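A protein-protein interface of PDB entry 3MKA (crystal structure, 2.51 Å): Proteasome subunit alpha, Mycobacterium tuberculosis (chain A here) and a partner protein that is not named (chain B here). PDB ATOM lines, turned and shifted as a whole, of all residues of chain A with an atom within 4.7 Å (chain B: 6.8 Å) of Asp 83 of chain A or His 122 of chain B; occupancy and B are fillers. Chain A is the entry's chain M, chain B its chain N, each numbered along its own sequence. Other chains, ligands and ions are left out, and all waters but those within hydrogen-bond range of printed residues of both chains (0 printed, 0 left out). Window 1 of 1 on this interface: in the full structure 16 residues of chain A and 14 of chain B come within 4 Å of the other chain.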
ATOM      1  N   TYR A  57      -7.433 -17.442   7.204  1.00  0.00           N
ATOM      2  CA  TYR A  57      -8.417 -16.553   7.762  1.00  0.00           C
ATOM      3  C   TYR A  57      -8.896 -15.555   6.682  1.00  0.00           C
ATOM      4  O   TYR A  57      -8.575 -15.673   5.497  1.00  0.00           O
ATOM      5  CB  TYR A  57      -7.832 -15.809   8.980  1.00  0.00           C
ATOM      6  CG  TYR A  57      -8.859 -15.510  10.070  1.00  0.00           C
ATOM      7  CD1 TYR A  57      -9.588 -16.540  10.689  1.00  0.00           C
ATOM      8  CD2 TYR A  57      -9.133 -14.208  10.437  1.00  0.00           C
ATOM      9  CE1 TYR A  57     -10.556 -16.266  11.619  1.00  0.00           C
ATOM     10  CE2 TYR A  57     -10.110 -13.918  11.383  1.00  0.00           C
ATOM     11  CZ  TYR A  57     -10.814 -14.937  11.957  1.00  0.00           C
ATOM     12  OH  TYR A  57     -11.811 -14.602  12.831  1.00  0.00           O
ATOM     13  N   ILE A  79      -5.475 -22.925  11.077  1.00  0.00           N
ATOM     14  CA  ILE A  79      -6.848 -22.577  10.983  1.00  0.00           C
ATOM     15  C   ILE A  79      -7.460 -22.622  12.408  1.00  0.00           C
ATOM     16  O   ILE A  79      -8.276 -21.789  12.743  1.00  0.00           O
ATOM     17  CB  ILE A  79      -7.546 -23.551  10.084  1.00  0.00           C
ATOM     18  CG1 ILE A  79      -7.179 -23.206   8.645  1.00  0.00           C
ATOM     19  CG2 ILE A  79      -9.100 -23.556  10.385  1.00  0.00           C
ATOM     20  CD1 ILE A  79      -7.691 -24.227   7.662  1.00  0.00           C
ATOM     21  N   GLN A  80      -7.045 -23.567  13.250  1.00  0.00           N
ATOM     22  CA  GLN A  80      -7.564 -23.612  14.621  1.00  0.00           C
ATOM     23  C   GLN A  80      -7.096 -22.439  15.402  1.00  0.00           C
ATOM     24  O   GLN A  80      -7.863 -21.849  16.135  1.00  0.00           O
ATOM     25  CB  GLN A  80      -7.143 -24.874  15.342  1.00  0.00           C
ATOM     26  CG  GLN A  80      -7.752 -26.061  14.679  1.00  0.00           C
ATOM     27  CD  GLN A  80      -7.277 -27.342  15.269  1.00  0.00           C
ATOM     28  OE1 GLN A  80      -6.166 -27.414  15.791  1.00  0.00           O
ATOM     29  NE2 GLN A  80      -8.102 -28.384  15.177  1.00  0.00           N
ATOM     30  N   PHE A  81      -5.838 -22.079  15.238  1.00  0.00           N
ATOM     31  CA  PHE A  81      -5.318 -20.947  15.962  1.00  0.00           C
ATOM     32  C   PHE A  81      -5.977 -19.624  15.553  1.00  0.00           C
ATOM     33  O   PHE A  81      -6.285 -18.796  16.398  1.00  0.00           O
ATOM     34  CB  PHE A  81      -3.828 -20.862  15.760  1.00  0.00           C
ATOM     35  CG  PHE A  81      -3.198 -19.638  16.387  1.00  0.00           C
ATOM     36  CD1 PHE A  81      -2.695 -19.686  17.675  1.00  0.00           C
ATOM     37  CD2 PHE A  81      -3.097 -18.431  15.660  1.00  0.00           C
ATOM     38  CE1 PHE A  81      -2.084 -18.556  18.260  1.00  0.00           C
ATOM     39  CE2 PHE A  81      -2.478 -17.266  16.239  1.00  0.00           C
ATOM     40  CZ  PHE A  81      -1.973 -17.352  17.550  1.00  0.00           C
ATOM     41  N   ALA A  82      -6.184 -19.419  14.271  1.00  0.00           N
ATOM     42  CA  ALA A  82      -6.787 -18.183  13.820  1.00  0.00           C
ATOM     43  C   ALA A  82      -8.268 -18.045  14.190  1.00  0.00           C
ATOM     44  O   ALA A  82      -8.701 -16.961  14.610  1.00  0.00           O
ATOM     45  CB  ALA A  82      -6.661 -18.054  12.342  1.00  0.00           C
ATOM     46  N   ASP A  83      -9.047 -19.111  13.972  1.00  0.00           N
ATOM     47  CA  ASP A  83     -10.444 -19.106  14.313  1.00  0.00           C
ATOM     48  C   ASP A  83     -10.582 -18.837  15.820  1.00  0.00           C
ATOM     49  O   ASP A  83     -11.409 -18.005  16.215  1.00  0.00           O
ATOM     50  CB  ASP A  83     -11.063 -20.438  13.929  1.00  0.00           C
ATOM     51  CG  ASP A  83     -11.488 -20.484  12.460  1.00  0.00           C
ATOM     52  OD1 ASP A  83     -11.359 -19.436  11.802  1.00  0.00           O
ATOM     53  OD2 ASP A  83     -11.954 -21.555  11.965  1.00  0.00           O
ATOM     54  N   THR A  84      -9.755 -19.490  16.643  1.00  0.00           N
ATOM     55  CA  THR A  84      -9.816 -19.296  18.079  1.00  0.00           C
ATOM     56  C   THR A  84      -9.537 -17.865  18.496  1.00  0.00           C
ATOM     57  O   THR A  84     -10.279 -17.278  19.309  1.00  0.00           O
ATOM     58  CB  THR A  84      -8.869 -20.255  18.795  1.00  0.00           C
ATOM     59  OG1 THR A  84      -9.346 -21.591  18.588  1.00  0.00           O
ATOM     60  CG2 THR A  84      -8.815 -19.986  20.277  1.00  0.00           C
ATOM     61  N   ARG A  85      -8.514 -17.266  17.926  1.00  0.00           N
ATOM     62  CA  ARG A  85      -8.202 -15.901  18.319  1.00  0.00           C
ATOM     63  C   ARG A  85      -9.239 -14.924  17.814  1.00  0.00           C
ATOM     64  O   ARG A  85      -9.529 -13.913  18.435  1.00  0.00           O
ATOM     65  CB  ARG A  85      -6.821 -15.478  17.814  1.00  0.00           C
ATOM     66  CG  ARG A  85      -5.692 -16.442  18.229  1.00  0.00           C
ATOM     67  CD  ARG A  85      -4.954 -15.967  19.474  1.00  0.00           C
ATOM     68  NE  ARG A  85      -4.351 -14.654  19.235  1.00  0.00           N
ATOM     69  CZ  ARG A  85      -3.232 -14.254  19.826  1.00  0.00           C
ATOM     70  NH1 ARG A  85      -2.608 -15.072  20.682  1.00  0.00           N
ATOM     71  NH2 ARG A  85      -2.754 -13.043  19.565  1.00  0.00           N
ATOM     72  N   GLY A  86      -9.827 -15.219  16.689  1.00  0.00           N
ATOM     73  CA  GLY A  86     -10.805 -14.288  16.178  1.00  0.00           C
ATOM     74  C   GLY A  86     -12.102 -14.352  16.964  1.00  0.00           C
ATOM     75  O   GLY A  86     -12.871 -13.401  16.943  1.00  0.00           O
ATOM     76  N   TYR A  87     -12.332 -15.475  17.648  1.00  0.00           N
ATOM     77  CA  TYR A  87     -13.510 -15.694  18.444  1.00  0.00           C
ATOM     78  C   TYR A  87     -13.289 -15.048  19.784  1.00  0.00           C
ATOM     79  O   TYR A  87     -14.151 -14.348  20.247  1.00  0.00           O
ATOM     80  CB  TYR A  87     -13.740 -17.166  18.639  1.00  0.00           C
ATOM     81  CG  TYR A  87     -15.052 -17.469  19.270  1.00  0.00           C
ATOM     82  CD1 TYR A  87     -16.246 -17.202  18.599  1.00  0.00           C
ATOM     83  CD2 TYR A  87     -15.111 -18.004  20.569  1.00  0.00           C
ATOM     84  CE1 TYR A  87     -17.472 -17.455  19.213  1.00  0.00           C
ATOM     85  CE2 TYR A  87     -16.309 -18.260  21.174  1.00  0.00           C
ATOM     86  CZ  TYR A  87     -17.486 -17.982  20.494  1.00  0.00           C
ATOM     87  OH  TYR A  87     -18.693 -18.233  21.100  1.00  0.00           O
ATOM     88  N   SER B  23     -13.024 -32.008  12.892  1.00  0.00           N
ATOM     89  CA  SER B  23     -12.866 -30.719  12.250  1.00  0.00           C
ATOM     90  C   SER B  23     -13.932 -29.753  12.805  1.00  0.00           C
ATOM     91  O   SER B  23     -14.481 -28.930  12.073  1.00  0.00           O
ATOM     92  CB  SER B  23     -13.061 -30.894  10.743  1.00  0.00           C
ATOM     93  OG  SER B  23     -12.263 -31.980  10.314  1.00  0.00           O
ATOM     94  N   SER B  24     -14.212 -29.865  14.098  1.00  0.00           N
ATOM     95  CA  SER B  24     -15.214 -29.044  14.752  1.00  0.00           C
ATOM     96  C   SER B  24     -14.611 -27.943  15.592  1.00  0.00           C
ATOM     97  O   SER B  24     -13.888 -28.210  16.567  1.00  0.00           O
ATOM     98  CB  SER B  24     -16.107 -29.903  15.655  1.00  0.00           C
ATOM     99  OG  SER B  24     -16.978 -29.098  16.437  1.00  0.00           O
ATOM    100  N   PHE B  25     -14.940 -26.704  15.294  1.00  0.00           N
ATOM    101  CA  PHE B  25     -14.385 -25.624  16.072  1.00  0.00           C
ATOM    102  C   PHE B  25     -14.808 -25.775  17.518  1.00  0.00           C
ATOM    103  O   PHE B  25     -14.032 -25.532  18.423  1.00  0.00           O
ATOM    104  CB  PHE B  25     -14.845 -24.284  15.536  1.00  0.00           C
ATOM    105  CG  PHE B  25     -14.254 -23.134  16.258  1.00  0.00           C
ATOM    106  CD1 PHE B  25     -12.895 -23.047  16.428  1.00  0.00           C
ATOM    107  CD2 PHE B  25     -15.049 -22.140  16.770  1.00  0.00           C
ATOM    108  CE1 PHE B  25     -12.349 -22.005  17.089  1.00  0.00           C
ATOM    109  CE2 PHE B  25     -14.501 -21.090  17.433  1.00  0.00           C
ATOM    110  CZ  PHE B  25     -13.152 -21.021  17.594  1.00  0.00           C
ATOM    111  N   THR B  26     -16.051 -26.184  17.719  1.00  0.00           N
ATOM    112  CA  THR B  26     -16.604 -26.379  19.047  1.00  0.00           C
ATOM    113  C   THR B  26     -15.910 -27.456  19.850  1.00  0.00           C
ATOM    114  O   THR B  26     -15.669 -27.289  21.032  1.00  0.00           O
ATOM    115  CB  THR B  26     -18.067 -26.737  18.954  1.00  0.00           C
ATOM    116  OG1 THR B  26     -18.809 -25.558  18.649  1.00  0.00           O
ATOM    117  CG2 THR B  26     -18.547 -27.303  20.258  1.00  0.00           C
ATOM    118  N   PHE B  28     -12.872 -28.400  19.467  1.00  0.00           N
ATOM    119  CA  PHE B  28     -11.551 -27.908  19.781  1.00  0.00           C
ATOM    120  C   PHE B  28     -11.576 -27.055  21.027  1.00  0.00           C
ATOM    121  O   PHE B  28     -10.721 -27.183  21.881  1.00  0.00           O
ATOM    122  CB  PHE B  28     -11.028 -27.083  18.617  1.00  0.00           C
ATOM    123  CG  PHE B  28      -9.603 -26.651  18.768  1.00  0.00           C
ATOM    124  CD1 PHE B  28      -8.578 -27.555  18.648  1.00  0.00           C
ATOM    125  CD2 PHE B  28      -9.288 -25.334  19.001  1.00  0.00           C
ATOM    126  CE1 PHE B  28      -7.289 -27.160  18.776  1.00  0.00           C
ATOM    127  CE2 PHE B  28      -7.998 -24.947  19.127  1.00  0.00           C
ATOM    128  CZ  PHE B  28      -7.000 -25.862  19.012  1.00  0.00           C
ATOM    129  N   LEU B  29     -12.560 -26.176  21.136  1.00  0.00           N
ATOM    130  CA  LEU B  29     -12.672 -25.346  22.319  1.00  0.00           C
ATOM    131  C   LEU B  29     -12.960 -26.193  23.534  1.00  0.00           C
ATOM    132  O   LEU B  29     -12.384 -26.006  24.591  1.00  0.00           O
ATOM    133  CB  LEU B  29     -13.777 -24.316  22.157  1.00  0.00           C
ATOM    134  CG  LEU B  29     -13.593 -23.321  21.028  1.00  0.00           C
ATOM    135  CD1 LEU B  29     -14.417 -22.095  21.279  1.00  0.00           C
ATOM    136  CD2 LEU B  29     -12.144 -22.967  20.929  1.00  0.00           C
ATOM    137  N   ALA B 117     -21.322 -19.564  13.066  1.00  0.00           N
ATOM    138  CA  ALA B 117     -20.826 -19.156  11.771  1.00  0.00           C
ATOM    139  C   ALA B 117     -19.366 -19.523  11.684  1.00  0.00           C
ATOM    140  O   ALA B 117     -18.898 -19.898  10.625  1.00  0.00           O
ATOM    141  CB  ALA B 117     -21.024 -17.662  11.555  1.00  0.00           C
ATOM    142  N   VAL B 118     -18.652 -19.408  12.791  1.00  0.00           N
ATOM    143  CA  VAL B 118     -17.270 -19.782  12.808  1.00  0.00           C
ATOM    144  C   VAL B 118     -17.177 -21.305  12.591  1.00  0.00           C
ATOM    145  O   VAL B 118     -16.408 -21.786  11.766  1.00  0.00           O
ATOM    146  CB  VAL B 118     -16.646 -19.366  14.145  1.00  0.00           C
ATOM    147  CG1 VAL B 118     -15.356 -20.087  14.366  1.00  0.00           C
ATOM    148  CG2 VAL B 118     -16.432 -17.871  14.122  1.00  0.00           C
ATOM    149  N   GLU B 119     -17.975 -22.054  13.316  1.00  0.00           N
ATOM    150  CA  GLU B 119     -17.971 -23.505  13.187  1.00  0.00           C
ATOM    151  C   GLU B 119     -18.188 -23.953  11.722  1.00  0.00           C
ATOM    152  O   GLU B 119     -17.555 -24.905  11.228  1.00  0.00           O
ATOM    153  CB  GLU B 119     -19.075 -24.116  14.056  1.00  0.00           C
ATOM    154  CG  GLU B 119     -19.348 -25.583  13.817  1.00  0.00           C
ATOM    155  CD  GLU B 119     -18.687 -26.466  14.870  1.00  0.00           C
ATOM    156  OE1 GLU B 119     -17.872 -25.904  15.656  1.00  0.00           O
ATOM    157  OE2 GLU B 119     -18.962 -27.707  14.918  1.00  0.00           O
ATOM    158  N   LEU B 120     -19.097 -23.277  11.039  1.00  0.00           N
ATOM    159  CA  LEU B 120     -19.354 -23.622   9.664  1.00  0.00           C
ATOM    160  C   LEU B 120     -18.150 -23.339   8.743  1.00  0.00           C
ATOM    161  O   LEU B 120     -17.770 -24.211   7.983  1.00  0.00           O
ATOM    162  CB  LEU B 120     -20.563 -22.851   9.179  1.00  0.00           C
ATOM    163  CG  LEU B 120     -21.861 -23.648   8.928  1.00  0.00           C
ATOM    164  CD1 LEU B 120     -22.124 -24.744   9.997  1.00  0.00           C
ATOM    165  CD2 LEU B 120     -23.004 -22.652   8.867  1.00  0.00           C
ATOM    166  N   GLU B 121     -17.569 -22.137   8.824  1.00  0.00           N
ATOM    167  CA  GLU B 121     -16.455 -21.725   7.996  1.00  0.00           C
ATOM    168  C   GLU B 121     -15.190 -22.475   8.367  1.00  0.00           C
ATOM    169  O   GLU B 121     -14.339 -22.705   7.537  1.00  0.00           O
ATOM    170  CB  GLU B 121     -16.248 -20.226   8.108  1.00  0.00           C
ATOM    171  CG  GLU B 121     -15.230 -19.720   7.172  1.00  0.00           C
ATOM    172  CD  GLU B 121     -15.149 -18.213   7.131  1.00  0.00           C
ATOM    173  OE1 GLU B 121     -16.058 -17.601   6.511  1.00  0.00           O
ATOM    174  OE2 GLU B 121     -14.171 -17.662   7.721  1.00  0.00           O
ATOM    175  N   HIS B 122     -15.076 -22.890   9.609  1.00  0.00           N
ATOM    176  CA  HIS B 122     -13.913 -23.645  10.025  1.00  0.00           C
ATOM    177  C   HIS B 122     -13.887 -25.004   9.296  1.00  0.00           C
ATOM    178  O   HIS B 122     -12.840 -25.415   8.777  1.00  0.00           O
ATOM    179  CB  HIS B 122     -14.023 -23.820  11.504  1.00  0.00           C
ATOM    180  CG  HIS B 122     -12.886 -24.523  12.158  1.00  0.00           C
ATOM    181  ND1 HIS B 122     -11.778 -23.852  12.624  1.00  0.00           N
ATOM    182  CD2 HIS B 122     -12.757 -25.806  12.583  1.00  0.00           C
ATOM    183  CE1 HIS B 122     -11.007 -24.687  13.316  1.00  0.00           C
ATOM    184  NE2 HIS B 122     -11.582 -25.881  13.306  1.00  0.00           N
ATOM    185  N   TYR B 123     -15.025 -25.699   9.244  1.00  0.00           N
ATOM    186  CA  TYR B 123     -15.076 -26.995   8.575  1.00  0.00           C
ATOM    187  C   TYR B 123     -14.742 -26.808   7.103  1.00  0.00           C
ATOM    188  O   TYR B 123     -14.054 -27.610   6.521  1.00  0.00           O
ATOM    189  CB  TYR B 123     -16.460 -27.627   8.655  1.00  0.00           C
ATOM    190  CG  TYR B 123     -16.566 -29.022   8.018  1.00  0.00           C
ATOM    191  CD1 TYR B 123     -16.352 -30.173   8.779  1.00  0.00           C
ATOM    192  CD2 TYR B 123     -16.898 -29.181   6.647  1.00  0.00           C
ATOM    193  CE1 TYR B 123     -16.465 -31.463   8.197  1.00  0.00           C
ATOM    194  CE2 TYR B 123     -17.006 -30.453   6.045  1.00  0.00           C
ATOM    195  CZ  TYR B 123     -16.785 -31.590   6.824  1.00  0.00           C
ATOM    196  OH  TYR B 123     -16.862 -32.834   6.232  1.00  0.00           O
ATOM    197  N   GLU B 124     -15.240 -25.748   6.504  1.00  0.00           N
ATOM    198  CA  GLU B 124     -14.972 -25.523   5.115  1.00  0.00           C
ATOM    199  C   GLU B 124     -13.504 -25.270   4.794  1.00  0.00           C
ATOM    200  O   GLU B 124     -13.037 -25.722   3.768  1.00  0.00           O
ATOM    201  CB  GLU B 124     -15.780 -24.367   4.604  1.00  0.00           C
ATOM    202  CG  GLU B 124     -15.566 -24.206   3.158  1.00  0.00           C
ATOM    203  CD  GLU B 124     -16.300 -23.031   2.619  1.00  0.00           C
ATOM    204  OE1 GLU B 124     -16.035 -21.904   3.068  1.00  0.00           O
ATOM    205  OE2 GLU B 124     -17.152 -23.236   1.743  1.00  0.00           O
ATOM    206  N   LYS B 125     -12.792 -24.532   5.635  1.00  0.00           N
ATOM    207  CA  LYS B 125     -11.398 -24.309   5.416  1.00  0.00           C
ATOM    208  C   LYS B 125     -10.609 -25.552   5.691  1.00  0.00           C
ATOM    209  O   LYS B 125      -9.682 -25.831   4.935  1.00  0.00           O
ATOM    210  CB  LYS B 125     -10.889 -23.210   6.272  1.00  0.00           C
ATOM    211  CG  LYS B 125     -11.424 -21.865   5.787  1.00  0.00           C
ATOM    212  CD  LYS B 125     -10.852 -20.700   6.596  1.00  0.00           C
ATOM    213  CE  LYS B 125     -11.306 -20.732   8.074  1.00  0.00           C
ATOM    214  NZ  LYS B 125     -10.902 -19.462   8.740  1.00  0.00           N
ATOM    215  N   LEU B 126     -10.958 -26.336   6.704  1.00  0.00           N
ATOM    216  CA  LEU B 126     -10.203 -27.546   6.948  1.00  0.00           C
ATOM    217  C   LEU B 126     -10.433 -28.609   5.892  1.00  0.00           C
ATOM    218  O   LEU B 126      -9.515 -29.351   5.549  1.00  0.00           O
ATOM    219  CB  LEU B 126     -10.595 -28.168   8.253  1.00  0.00           C
ATOM    220  CG  LEU B 126     -10.275 -27.354   9.483  1.00  0.00           C
ATOM    221  CD1 LEU B 126     -10.917 -28.040  10.670  1.00  0.00           C
ATOM    222  CD2 LEU B 126      -8.746 -27.220   9.634  1.00  0.00           C
ATOM    223  N   GLU B 127     -11.660 -28.725   5.403  1.00  0.00           N
ATOM    224  CA  GLU B 127     -11.985 -29.780   4.451  1.00  0.00           C
ATOM    225  C   GLU B 127     -12.129 -29.312   3.052  1.00  0.00           C
ATOM    226  O   GLU B 127     -12.389 -30.099   2.176  1.00  0.00           O
ATOM    227  CB  GLU B 127     -13.283 -30.501   4.844  1.00  0.00           C
ATOM    228  CG  GLU B 127     -13.236 -31.085   6.230  1.00  0.00           C
ATOM    229  CD  GLU B 127     -12.126 -32.118   6.408  1.00  0.00           C
ATOM    230  OE1 GLU B 127     -11.880 -32.913   5.459  1.00  0.00           O
ATOM    231  OE2 GLU B 127     -11.521 -32.148   7.496  1.00  0.00           O
ATOM    232  N   GLY B 128     -12.012 -28.023   2.839  1.00  0.00           N
ATOM    233  CA  GLY B 128     -12.123 -27.523   1.477  1.00  0.00           C
ATOM    234  C   GLY B 128     -13.502 -27.587   0.875  1.00  0.00           C
ATOM    235  O   GLY B 128     -13.736 -27.210  -0.247  1.00  0.00           O
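OD1 of Asp 83 of chain A lies within salt-bridge range of NZ of Lys 125 of chain B (3.1 Å). OD2 of Asp 83 of chain A sits close to ND1 of His 122 of chain B (2.4 Å).
The backbone carbonyl oxygen of Gln 80 of chain A lies within hydrogen-bond range of the side-chain hydroxyl of Thr 84 of chain A, 2.9 Å away. OE1 of Glu 119 of chain B sits at hydrogen-bond distance from N of Phe 25 of chain B, at 3.1 Å. OE2 of Glu 121 of chain B lies within salt-bridge range of NZ of Lys 125 of chain B, 3.9 Å away.
Among the printed residues, merely in contact across the chains: Tyr 57 of chain A with Lys 125 of chain B (3.8 Å), Ile 79 of chain A with His 122 of chain B (3.5 Å), Ile 79 of chain A with Lys 125 of chain B (3.6 Å), Ile 79 of chain A with Leu 126 of chain B (3.7 Å), Gln 80 of chain A with Phe 28 of chain B (3.2 Å), Gln 80 of chain A with His 122 of chain B (3.8 Å), Asp 83 of chain A with Phe 25 of chain B (3.7 Å), Thr 84 of chain A with Phe 25 of chain B (3.4 Å), Thr 84 of chain A with Phe 28 of chain B (3.7 Å) and Thr 84 of chain A with Leu 29 of chain B (3.9 Å).
Of the printed residues of chain B, Tyr 57 of chain A touches Lys 125 (3.8 Å). Of the printed residues of chain B, Gln 80 of chain A touches Phe 28 and His 122. Of chain B, only Phe 25 (3.7 Å), His 122 (2.4 Å) and Lys 125 (3.1 Å) come within 4 Å of Asp 83 of chain A. His 122 of chain B touches three residues of chain A. Tyr 123 of chain B touches none of the printed residues of chain A.
Of the 18 printed residues of chain B, 6 touch a printed residue of chain A. Printed residues of chain B that touch a printed residue of chain A: Phe 25, Phe 28, Leu 29, His 122, Lys 125 and Leu 126. Of the 10 printed residues of chain A, 5 touch a printed residue of chain B. Printed residues of chain A that touch a printed residue of chain B: Tyr 57, Ile 79, Gln 80, Asp 83 and Thr 84. Hydrophobic or aromatic side chains of chain A within 4 Å of the printed part of chain B: Tyr 57 and Ile 79. Among the printed residues, 12 pairs touch across the chains. Among the printed residues, Asp or Glu carboxylates within 4 Å of a Lys or Arg side-chain nitrogen of the other chain: Asp 83 of chain A with Lys 125 of chain B (3.1 Å).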
